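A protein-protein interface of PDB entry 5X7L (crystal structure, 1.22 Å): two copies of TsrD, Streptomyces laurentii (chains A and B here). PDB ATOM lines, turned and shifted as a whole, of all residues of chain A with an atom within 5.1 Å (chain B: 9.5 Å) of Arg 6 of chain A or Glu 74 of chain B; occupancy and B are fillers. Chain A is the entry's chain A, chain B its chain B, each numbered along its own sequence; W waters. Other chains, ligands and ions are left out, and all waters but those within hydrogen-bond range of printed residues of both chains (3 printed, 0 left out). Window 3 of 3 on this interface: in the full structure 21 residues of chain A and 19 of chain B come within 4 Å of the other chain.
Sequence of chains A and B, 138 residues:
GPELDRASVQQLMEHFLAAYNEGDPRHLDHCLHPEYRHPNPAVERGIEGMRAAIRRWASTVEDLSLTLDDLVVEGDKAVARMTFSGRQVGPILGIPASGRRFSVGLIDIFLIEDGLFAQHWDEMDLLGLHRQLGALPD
Positions printed for both chains: 4, 5, 6, 9, 71, 72 and 73.
NH2 of Arg 6 of chain A lies within hydrogen-bond range of O of Leu 71 of chain A.
The backbone carbonyl oxygen (O) of Val 72 of chain B sits at hydrogen-bond distance from the backbone NH (N) of Val 79 of chain B.
Water W2 lies within hydrogen-bond range of the backbone carbonyl oxygen of Val 73 of chain B and the backbone carbonyl oxygen of Val 73 of chain A.
Water W3 bridges NZ of Lys 77 of chain B (3.0 Å) and O of Leu 71 of chain A (3.3 Å).
Water W1 bridges the side-chain carboxylate of Glu 74 of chain B (3.0 Å) and the backbone carbonyl oxygen of Val 73 of chain A (3.3 Å).
Of chain B, only Glu 74 (2.5 Å) comes within 4 Å of Arg 6 of chain A.
Glu 74 of chain B touches just these residues of chain A: Arg 6, Leu 71, Val 72 and Val 73.
No residue of chain B comes within 4 Å of Asp 5 of chain A.
No residue of chain B comes within 4 Å of Val 9 of chain A.
Printed residues of chain A within 4 Å of Lys 77 of chain B: Val 72 (3.8 Å).
Printed residues of chain B within 4 Å of Leu 71 of chain A: Glu 74 (3.95 Å).
Printed residues of chain A within 4 Å of Val 79 of chain B: Val 72 (3.97 Å).
The nearest residue of chain B that does not touch Arg 6 of chain A is Lys 77 of chain B (7.4 Å).
Leu 71 of chain A touches Glu 74 of chain B (O to OE1, 3.95 Å).
CA of Val 72 of chain A touches OE1 of Glu 74 of chain B, at 3.5 Å.
CG2 of Val 72 of chain A touches CB of Lys 77 of chain B, 3.8 Å away.
Val 72 of chain A touches Val 79 of chain B (CG2 to CG2, 3.97 Å).
Of the 18 printed residues of chain B, 3 touch a printed residue of chain A.
Hydrophobic or aromatic side chains of chain B within 4 Å of the printed part of chain A: Val 79.
Of the 10 printed residues of chain A, 4 touch a printed residue of chain B.
Hydrophobic or aromatic side chains of chain A that line the printed part of chain B: Val 72.
Among the printed residues, Asp or Glu carboxylates within 4 Å of a Lys or Arg side-chain nitrogen of the other chain: Arg 6 of chain A with Glu 74 of chain B.
The guanidinium group (NE) of Arg 6 of chain A is in salt-bridge range of the side-chain carboxylate (OE2) of Glu 74 of chain B, 2.5 Å away.
N of Val 73 of chain A lies within hydrogen-bond range of OE1 of Glu 74 of chain B (2.9 Å).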
ATOM      1  N   LEU A   4      14.824  15.350  17.561  1.00  0.00           N
ATOM      2  CA  LEU A   4      14.347  14.133  18.209  1.00  0.00           C
ATOM      3  C   LEU A   4      13.211  13.512  17.419  1.00  0.00           C
ATOM      4  O   LEU A   4      12.273  14.203  17.019  1.00  0.00           O
ATOM      5  CB  LEU A   4      13.876  14.408  19.643  1.00  0.00           C
ATOM      6  CG  LEU A   4      14.957  14.464  20.721  1.00  0.00           C
ATOM      7  CD1 LEU A   4      14.319  14.549  22.098  1.00  0.00           C
ATOM      8  CD2 LEU A   4      15.880  13.258  20.642  1.00  0.00           C
ATOM      9  N   ASP A   5      13.304  12.202  17.194  1.00  0.00           N
ATOM     10  CA  ASP A   5      12.189  11.440  16.653  1.00  0.00           C
ATOM     11  C   ASP A   5      11.012  11.577  17.609  1.00  0.00           C
ATOM     12  O   ASP A   5      11.197  11.752  18.813  1.00  0.00           O
ATOM     13  CB  ASP A   5      12.566   9.968  16.474  1.00  0.00           C
ATOM     14  N   ARG A   6       9.802  11.511  17.073  1.00  0.00           N
ATOM     15  CA  ARG A   6       8.611  11.760  17.874  1.00  0.00           C
ATOM     16  C   ARG A   6       8.468  10.768  19.032  1.00  0.00           C
ATOM     17  O   ARG A   6       8.148  11.152  20.162  1.00  0.00           O
ATOM     18  CB  ARG A   6       7.366  11.712  17.002  1.00  0.00           C
ATOM     19  CG  ARG A   6       6.138  12.133  17.766  1.00  0.00           C
ATOM     20  CD  ARG A   6       4.859  11.939  16.989  1.00  0.00           C
ATOM     21  NE  ARG A   6       3.849  12.880  17.462  1.00  0.00           N
ATOM     22  CZ  ARG A   6       3.168  12.759  18.599  1.00  0.00           C
ATOM     23  NH1 ARG A   6       3.377  11.721  19.405  1.00  0.00           N
ATOM     24  NH2 ARG A   6       2.274  13.682  18.937  1.00  0.00           N
ATOM     25  N   ALA A   7       8.706   9.493  18.746  1.00  0.00           N
ATOM     26  CA  ALA A   7       8.687   8.461  19.777  1.00  0.00           C
ATOM     27  C   ALA A   7       9.683   8.789  20.890  1.00  0.00           C
ATOM     28  O   ALA A   7       9.447   8.473  22.056  1.00  0.00           O
ATOM     29  CB  ALA A   7       8.992   7.099  19.170  1.00  0.00           C
ATOM     30  N   SER A   8      10.791   9.433  20.532  1.00  0.00           N
ATOM     31  CA  SER A   8      11.779   9.841  21.526  1.00  0.00           C
ATOM     32  C   SER A   8      11.225  10.925  22.450  1.00  0.00           C
ATOM     33  O   SER A   8      11.498  10.919  23.646  1.00  0.00           O
ATOM     34  CB  SER A   8      13.066  10.327  20.855  1.00  0.00           C
ATOM     35  OG  SER A   8      13.710   9.273  20.163  1.00  0.00           O
ATOM     36  N   VAL A   9      10.444  11.850  21.901  1.00  0.00           N
ATOM     37  CA  VAL A   9       9.814  12.880  22.723  1.00  0.00           C
ATOM     38  C   VAL A   9       8.781  12.250  23.663  1.00  0.00           C
ATOM     39  O   VAL A   9       8.681  12.638  24.826  1.00  0.00           O
ATOM     40  CB  VAL A   9       9.158  13.981  21.869  1.00  0.00           C
ATOM     41  CG1 VAL A   9       8.445  14.989  22.759  1.00  0.00           C
ATOM     42  CG2 VAL A   9      10.204  14.677  21.007  1.00  0.00           C
ATOM     43  N   GLN A  10       8.025  11.275  23.164  1.00  0.00           N
ATOM     44  CA  GLN A  10       7.091  10.531  24.011  1.00  0.00           C
ATOM     45  C   GLN A  10       7.814   9.898  25.197  1.00  0.00           C
ATOM     46  O   GLN A  10       7.310   9.918  26.319  1.00  0.00           O
ATOM     47  CB  GLN A  10       6.361   9.454  23.207  1.00  0.00           C
ATOM     48  CG  GLN A  10       5.466  10.005  22.112  1.00  0.00           C
ATOM     49  N   LEU A  71      -0.361  15.573  23.288  1.00  0.00           N
ATOM     50  CA  LEU A  71       1.033  15.870  22.996  1.00  0.00           C
ATOM     51  C   LEU A  71       1.136  16.301  21.539  1.00  0.00           C
ATOM     52  O   LEU A  71       0.667  15.600  20.641  1.00  0.00           O
ATOM     53  CB  LEU A  71       1.917  14.646  23.251  1.00  0.00           C
ATOM     54  CG  LEU A  71       3.418  14.793  22.976  1.00  0.00           C
ATOM     55  CD1 LEU A  71       4.066  15.781  23.933  1.00  0.00           C
ATOM     56  CD2 LEU A  71       4.101  13.439  23.070  1.00  0.00           C
ATOM     57  N   VAL A  72       1.744  17.463  21.315  1.00  0.00           N
ATOM     58  CA  VAL A  72       1.945  18.009  19.974  1.00  0.00           C
ATOM     59  C   VAL A  72       3.435  18.289  19.810  1.00  0.00           C
ATOM     60  O   VAL A  72       4.022  19.014  20.616  1.00  0.00           O
ATOM     61  CB  VAL A  72       1.122  19.296  19.756  1.00  0.00           C
ATOM     62  CG1 VAL A  72       1.292  19.821  18.332  1.00  0.00           C
ATOM     63  CG2 VAL A  72      -0.346  19.038  20.055  1.00  0.00           C
ATOM     64  N   VAL A  73       4.042  17.703  18.782  1.00  0.00           N
ATOM     65  CA  VAL A  73       5.488  17.758  18.609  1.00  0.00           C
ATOM     66  C   VAL A  73       5.845  18.307  17.235  1.00  0.00           C
ATOM     67  O   VAL A  73       5.310  17.857  16.221  1.00  0.00           O
ATOM     68  CB  VAL A  73       6.126  16.362  18.774  1.00  0.00           C
ATOM     69  CG1 VAL A  73       7.643  16.421  18.588  1.00  0.00           C
ATOM     70  CG2 VAL A  73       5.773  15.788  20.135  1.00  0.00           C
ATOM     71  N   GLU B   3      -2.866  17.345   7.606  1.00  0.00           N
ATOM     72  CA  GLU B   3      -3.379  17.610   6.242  1.00  0.00           C
ATOM     73  C   GLU B   3      -3.022  19.019   5.775  1.00  0.00           C
ATOM     74  O   GLU B   3      -2.545  19.196   4.655  1.00  0.00           O
ATOM     75  CB  GLU B   3      -4.892  17.380   6.180  1.00  0.00           C
ATOM     76  CG  GLU B   3      -5.557  17.847   4.893  1.00  0.00           C
ATOM     77  CD  GLU B   3      -6.199  19.216   5.028  1.00  0.00           C
ATOM     78  N   LEU B   4      -3.260  20.019   6.620  1.00  0.00           N
ATOM     79  CA  LEU B   4      -2.855  21.385   6.295  1.00  0.00           C
ATOM     80  C   LEU B   4      -1.345  21.541   6.373  1.00  0.00           C
ATOM     81  O   LEU B   4      -0.717  21.083   7.329  1.00  0.00           O
ATOM     82  CB  LEU B   4      -3.509  22.403   7.232  1.00  0.00           C
ATOM     83  CG  LEU B   4      -4.970  22.772   6.977  1.00  0.00           C
ATOM     84  CD1 LEU B   4      -5.351  23.939   7.871  1.00  0.00           C
ATOM     85  CD2 LEU B   4      -5.221  23.114   5.515  1.00  0.00           C
ATOM     86  N   ASP B   5      -0.772  22.193   5.366  1.00  0.00           N
ATOM     87  CA  ASP B   5       0.631  22.586   5.411  1.00  0.00           C
ATOM     88  C   ASP B   5       0.810  23.643   6.496  1.00  0.00           C
ATOM     89  O   ASP B   5      -0.155  24.287   6.915  1.00  0.00           O
ATOM     90  CB  ASP B   5       1.092  23.126   4.055  1.00  0.00           C
ATOM     91  N   ARG B   6       2.044  23.820   6.950  1.00  0.00           N
ATOM     92  CA  ARG B   6       2.322  24.739   8.048  1.00  0.00           C
ATOM     93  C   ARG B   6       2.003  26.188   7.688  1.00  0.00           C
ATOM     94  O   ARG B   6       1.469  26.943   8.507  1.00  0.00           O
ATOM     95  CB  ARG B   6       3.779  24.639   8.474  1.00  0.00           C
ATOM     96  CG  ARG B   6       4.056  25.454   9.709  1.00  0.00           C
ATOM     97  CD  ARG B   6       5.498  25.372  10.139  1.00  0.00           C
ATOM     98  NE  ARG B   6       5.556  25.395  11.592  1.00  0.00           N
ATOM     99  CZ  ARG B   6       5.442  26.490  12.337  1.00  0.00           C
ATOM    100  NH1 ARG B   6       5.284  27.683  11.772  1.00  0.00           N
ATOM    101  NH2 ARG B   6       5.493  26.384  13.657  1.00  0.00           N
ATOM    102  N   VAL B   9      -1.580  26.844   8.170  1.00  0.00           N
ATOM    103  CA  VAL B   9      -1.963  27.042   9.566  1.00  0.00           C
ATOM    104  C   VAL B   9      -1.571  28.448  10.021  1.00  0.00           C
ATOM    105  O   VAL B   9      -2.322  29.100  10.750  1.00  0.00           O
ATOM    106  CB  VAL B   9      -1.337  25.983  10.493  1.00  0.00           C
ATOM    107  CG1 VAL B   9      -1.699  26.261  11.947  1.00  0.00           C
ATOM    108  CG2 VAL B   9      -1.807  24.590  10.091  1.00  0.00           C
ATOM    109  N   LEU B  71       4.057  29.305  17.783  1.00  0.00           N
ATOM    110  CA  LEU B  71       3.124  28.436  17.081  1.00  0.00           C
ATOM    111  C   LEU B  71       3.794  27.084  16.875  1.00  0.00           C
ATOM    112  O   LEU B  71       4.924  27.020  16.385  1.00  0.00           O
ATOM    113  CB  LEU B  71       2.727  29.045  15.734  1.00  0.00           C
ATOM    114  CG  LEU B  71       1.784  28.223  14.851  1.00  0.00           C
ATOM    115  CD1 LEU B  71       0.412  28.078  15.494  1.00  0.00           C
ATOM    116  CD2 LEU B  71       1.668  28.852  13.470  1.00  0.00           C
ATOM    117  N   VAL B  72       3.108  26.017  17.274  1.00  0.00           N
ATOM    118  CA  VAL B  72       3.600  24.652  17.102  1.00  0.00           C
ATOM    119  C   VAL B  72       2.528  23.871  16.349  1.00  0.00           C
ATOM    120  O   VAL B  72       1.365  23.860  16.755  1.00  0.00           O
ATOM    121  CB  VAL B  72       3.907  23.981  18.460  1.00  0.00           C
ATOM    122  CG1 VAL B  72       4.459  22.575  18.258  1.00  0.00           C
ATOM    123  CG2 VAL B  72       4.891  24.826  19.259  1.00  0.00           C
ATOM    124  N   VAL B  73       2.921  23.226  15.254  1.00  0.00           N
ATOM    125  CA  VAL B  73       1.970  22.578  14.351  1.00  0.00           C
ATOM    126  C   VAL B  73       2.351  21.121  14.099  1.00  0.00           C
ATOM    127  O   VAL B  73       3.499  20.823  13.775  1.00  0.00           O
ATOM    128  CB  VAL B  73       1.894  23.313  12.995  1.00  0.00           C
ATOM    129  CG1 VAL B  73       0.914  22.624  12.053  1.00  0.00           C
ATOM    130  CG2 VAL B  73       1.501  24.768  13.204  1.00  0.00           C
ATOM    131  N   GLU B  74       1.381  20.221  14.248  1.00  0.00           N
ATOM    132  CA  GLU B  74       1.577  18.811  13.922  1.00  0.00           C
ATOM    133  C   GLU B  74       0.254  18.177  13.525  1.00  0.00           C
ATOM    134  O   GLU B  74      -0.694  18.176  14.311  1.00  0.00           O
ATOM    135  CB  GLU B  74       2.163  18.042  15.106  1.00  0.00           C
ATOM    136  CG  GLU B  74       2.467  16.585  14.779  1.00  0.00           C
ATOM    137  CD  GLU B  74       2.851  15.762  15.992  1.00  0.00           C
ATOM    138  OE1 GLU B  74       2.389  16.064  17.111  1.00  0.00           O
ATOM    139  OE2 GLU B  74       3.622  14.797  15.821  1.00  0.00           O
ATOM    140  N   GLY B  75       0.191  17.632  12.314  1.00  0.00           N
ATOM    141  CA  GLY B  75      -0.994  16.916  11.863  1.00  0.00           C
ATOM    142  C   GLY B  75      -2.235  17.788  11.918  1.00  0.00           C
ATOM    143  O   GLY B  75      -2.289  18.836  11.273  1.00  0.00           O
ATOM    144  N   ASP B  76      -3.224  17.371  12.705  1.00  0.00           N
ATOM    145  CA  ASP B  76      -4.462  18.140  12.843  1.00  0.00           C
ATOM    146  C   ASP B  76      -4.489  19.015  14.101  1.00  0.00           C
ATOM    147  O   ASP B  76      -5.561  19.399  14.563  1.00  0.00           O
ATOM    148  CB  ASP B  76      -5.691  17.213  12.792  1.00  0.00           C
ATOM    149  CG  ASP B  76      -5.742  16.209  13.936  1.00  0.00           C
ATOM    150  OD1 ASP B  76      -4.810  16.167  14.768  1.00  0.00           O
ATOM    151  OD2 ASP B  76      -6.732  15.448  13.993  1.00  0.00           O
ATOM    152  N   LYS B  77      -3.308  19.353  14.622  1.00  0.00           N
ATOM    153  CA  LYS B  77      -3.203  20.200  15.810  1.00  0.00           C
ATOM    154  C   LYS B  77      -2.375  21.453  15.553  1.00  0.00           C
ATOM    155  O   LYS B  77      -1.331  21.403  14.900  1.00  0.00           O
ATOM    156  CB  LYS B  77      -2.583  19.426  16.977  1.00  0.00           C
ATOM    157  CG  LYS B  77      -3.412  18.246  17.460  1.00  0.00           C
ATOM    158  CD  LYS B  77      -4.637  18.683  18.253  1.00  0.00           C
ATOM    159  CE  LYS B  77      -5.555  17.509  18.555  1.00  0.00           C
ATOM    160  NZ  LYS B  77      -4.872  16.439  19.332  1.00  0.00           N
ATOM    161  N   ALA B  78      -2.853  22.573  16.086  1.00  0.00           N
ATOM    162  CA  ALA B  78      -2.102  23.822  16.093  1.00  0.00           C
ATOM    163  C   ALA B  78      -2.108  24.384  17.503  1.00  0.00           C
ATOM    164  O   ALA B  78      -3.166  24.522  18.113  1.00  0.00           O
ATOM    165  CB  ALA B  78      -2.713  24.818  15.122  1.00  0.00           C
ATOM    166  N   VAL B  79      -0.925  24.697  18.019  1.00  0.00           N
ATOM    167  CA  VAL B  79      -0.792  25.269  19.351  1.00  0.00           C
ATOM    168  C   VAL B  79      -0.294  26.699  19.237  1.00  0.00           C
ATOM    169  O   VAL B  79       0.778  26.939  18.685  1.00  0.00           O
ATOM    170  CB  VAL B  79       0.188  24.468  20.223  1.00  0.00           C
ATOM    171  CG1 VAL B  79       0.251  25.067  21.622  1.00  0.00           C
ATOM    172  CG2 VAL B  79      -0.224  23.003  20.267  1.00  0.00           C
ATOM    173  N   ILE B 109      -4.839  25.212  22.138  1.00  0.00           N
ATOM    174  CA  ILE B 109      -4.611  24.081  21.251  1.00  0.00           C
ATOM    175  C   ILE B 109      -5.858  23.917  20.399  1.00  0.00           C
ATOM    176  O   ILE B 109      -6.944  23.708  20.931  1.00  0.00           O
ATOM    177  CB  ILE B 109      -4.332  22.783  22.029  1.00  0.00           C
ATOM    178  CG1 ILE B 109      -3.113  22.965  22.937  1.00  0.00           C
ATOM    179  CG2 ILE B 109      -4.134  21.621  21.062  1.00  0.00           C
ATOM    180  CD1 ILE B 109      -2.836  21.791  23.846  1.00  0.00           C
ATOM    181  N   PHE B 110      -5.699  24.021  19.082  1.00  0.00           N
ATOM    182  CA  PHE B 110      -6.808  23.878  18.146  1.00  0.00           C
ATOM    183  C   PHE B 110      -6.758  22.539  17.428  1.00  0.00           C
ATOM    184  O   PHE B 110      -5.689  22.081  17.020  1.00  0.00           O
ATOM    185  CB  PHE B 110      -6.772  24.972  17.083  1.00  0.00           C
ATOM    186  CG  PHE B 110      -6.966  26.360  17.613  1.00  0.00           C
ATOM    187  CD1 PHE B 110      -8.229  26.816  17.963  1.00  0.00           C
ATOM    188  CD2 PHE B 110      -5.889  27.228  17.725  1.00  0.00           C
ATOM    189  CE1 PHE B 110      -8.412  28.107  18.433  1.00  0.00           C
ATOM    190  CE2 PHE B 110      -6.068  28.520  18.198  1.00  0.00           C
ATOM    191  CZ  PHE B 110      -7.331  28.959  18.548  1.00  0.00           C
ATOM    192  N   LEU B 111      -7.931  21.934  17.267  1.00  0.00           N
ATOM    193  CA  LEU B 111      -8.123  20.779  16.398  1.00  0.00           C
ATOM    194  C   LEU B 111      -8.564  21.266  15.020  1.00  0.00           C
ATOM    195  O   LEU B 111      -9.509  22.045  14.908  1.00  0.00           O
ATOM    196  CB  LEU B 111      -9.182  19.845  16.986  1.00  0.00           C
ATOM    197  CG  LEU B 111      -9.568  18.602  16.178  1.00  0.00           C
ATOM    198  CD1 LEU B 111      -8.401  17.631  16.079  1.00  0.00           C
ATOM    199  CD2 LEU B 111     -10.787  17.930  16.801  1.00  0.00           C
ATOM    200  N   ILE B 112      -7.880  20.799  13.980  1.00  0.00           N
ATOM    201  CA  ILE B 112      -8.187  21.180  12.604  1.00  0.00           C
ATOM    202  C   ILE B 112      -9.068  20.121  11.940  1.00  0.00           C
ATOM    203  O   ILE B 112      -8.699  18.948  11.883  1.00  0.00           O
ATOM    204  CB  ILE B 112      -6.892  21.375  11.783  1.00  0.00           C
ATOM    205  CG1 ILE B 112      -6.009  22.448  12.432  1.00  0.00           C
ATOM    206  CG2 ILE B 112      -7.213  21.744  10.339  1.00  0.00           C
ATOM    207  CD1 ILE B 112      -4.567  22.417  11.975  1.00  0.00           C
HETATM  208  O   HOH W   1       6.494  15.054  14.968  1.00  0.00           O
HETATM  209  O   HOH W   2       5.087  18.537  13.509  1.00  0.00           O
HETATM  210  O   HOH W   3      -2.161  15.261  19.066  1.00  0.00           O
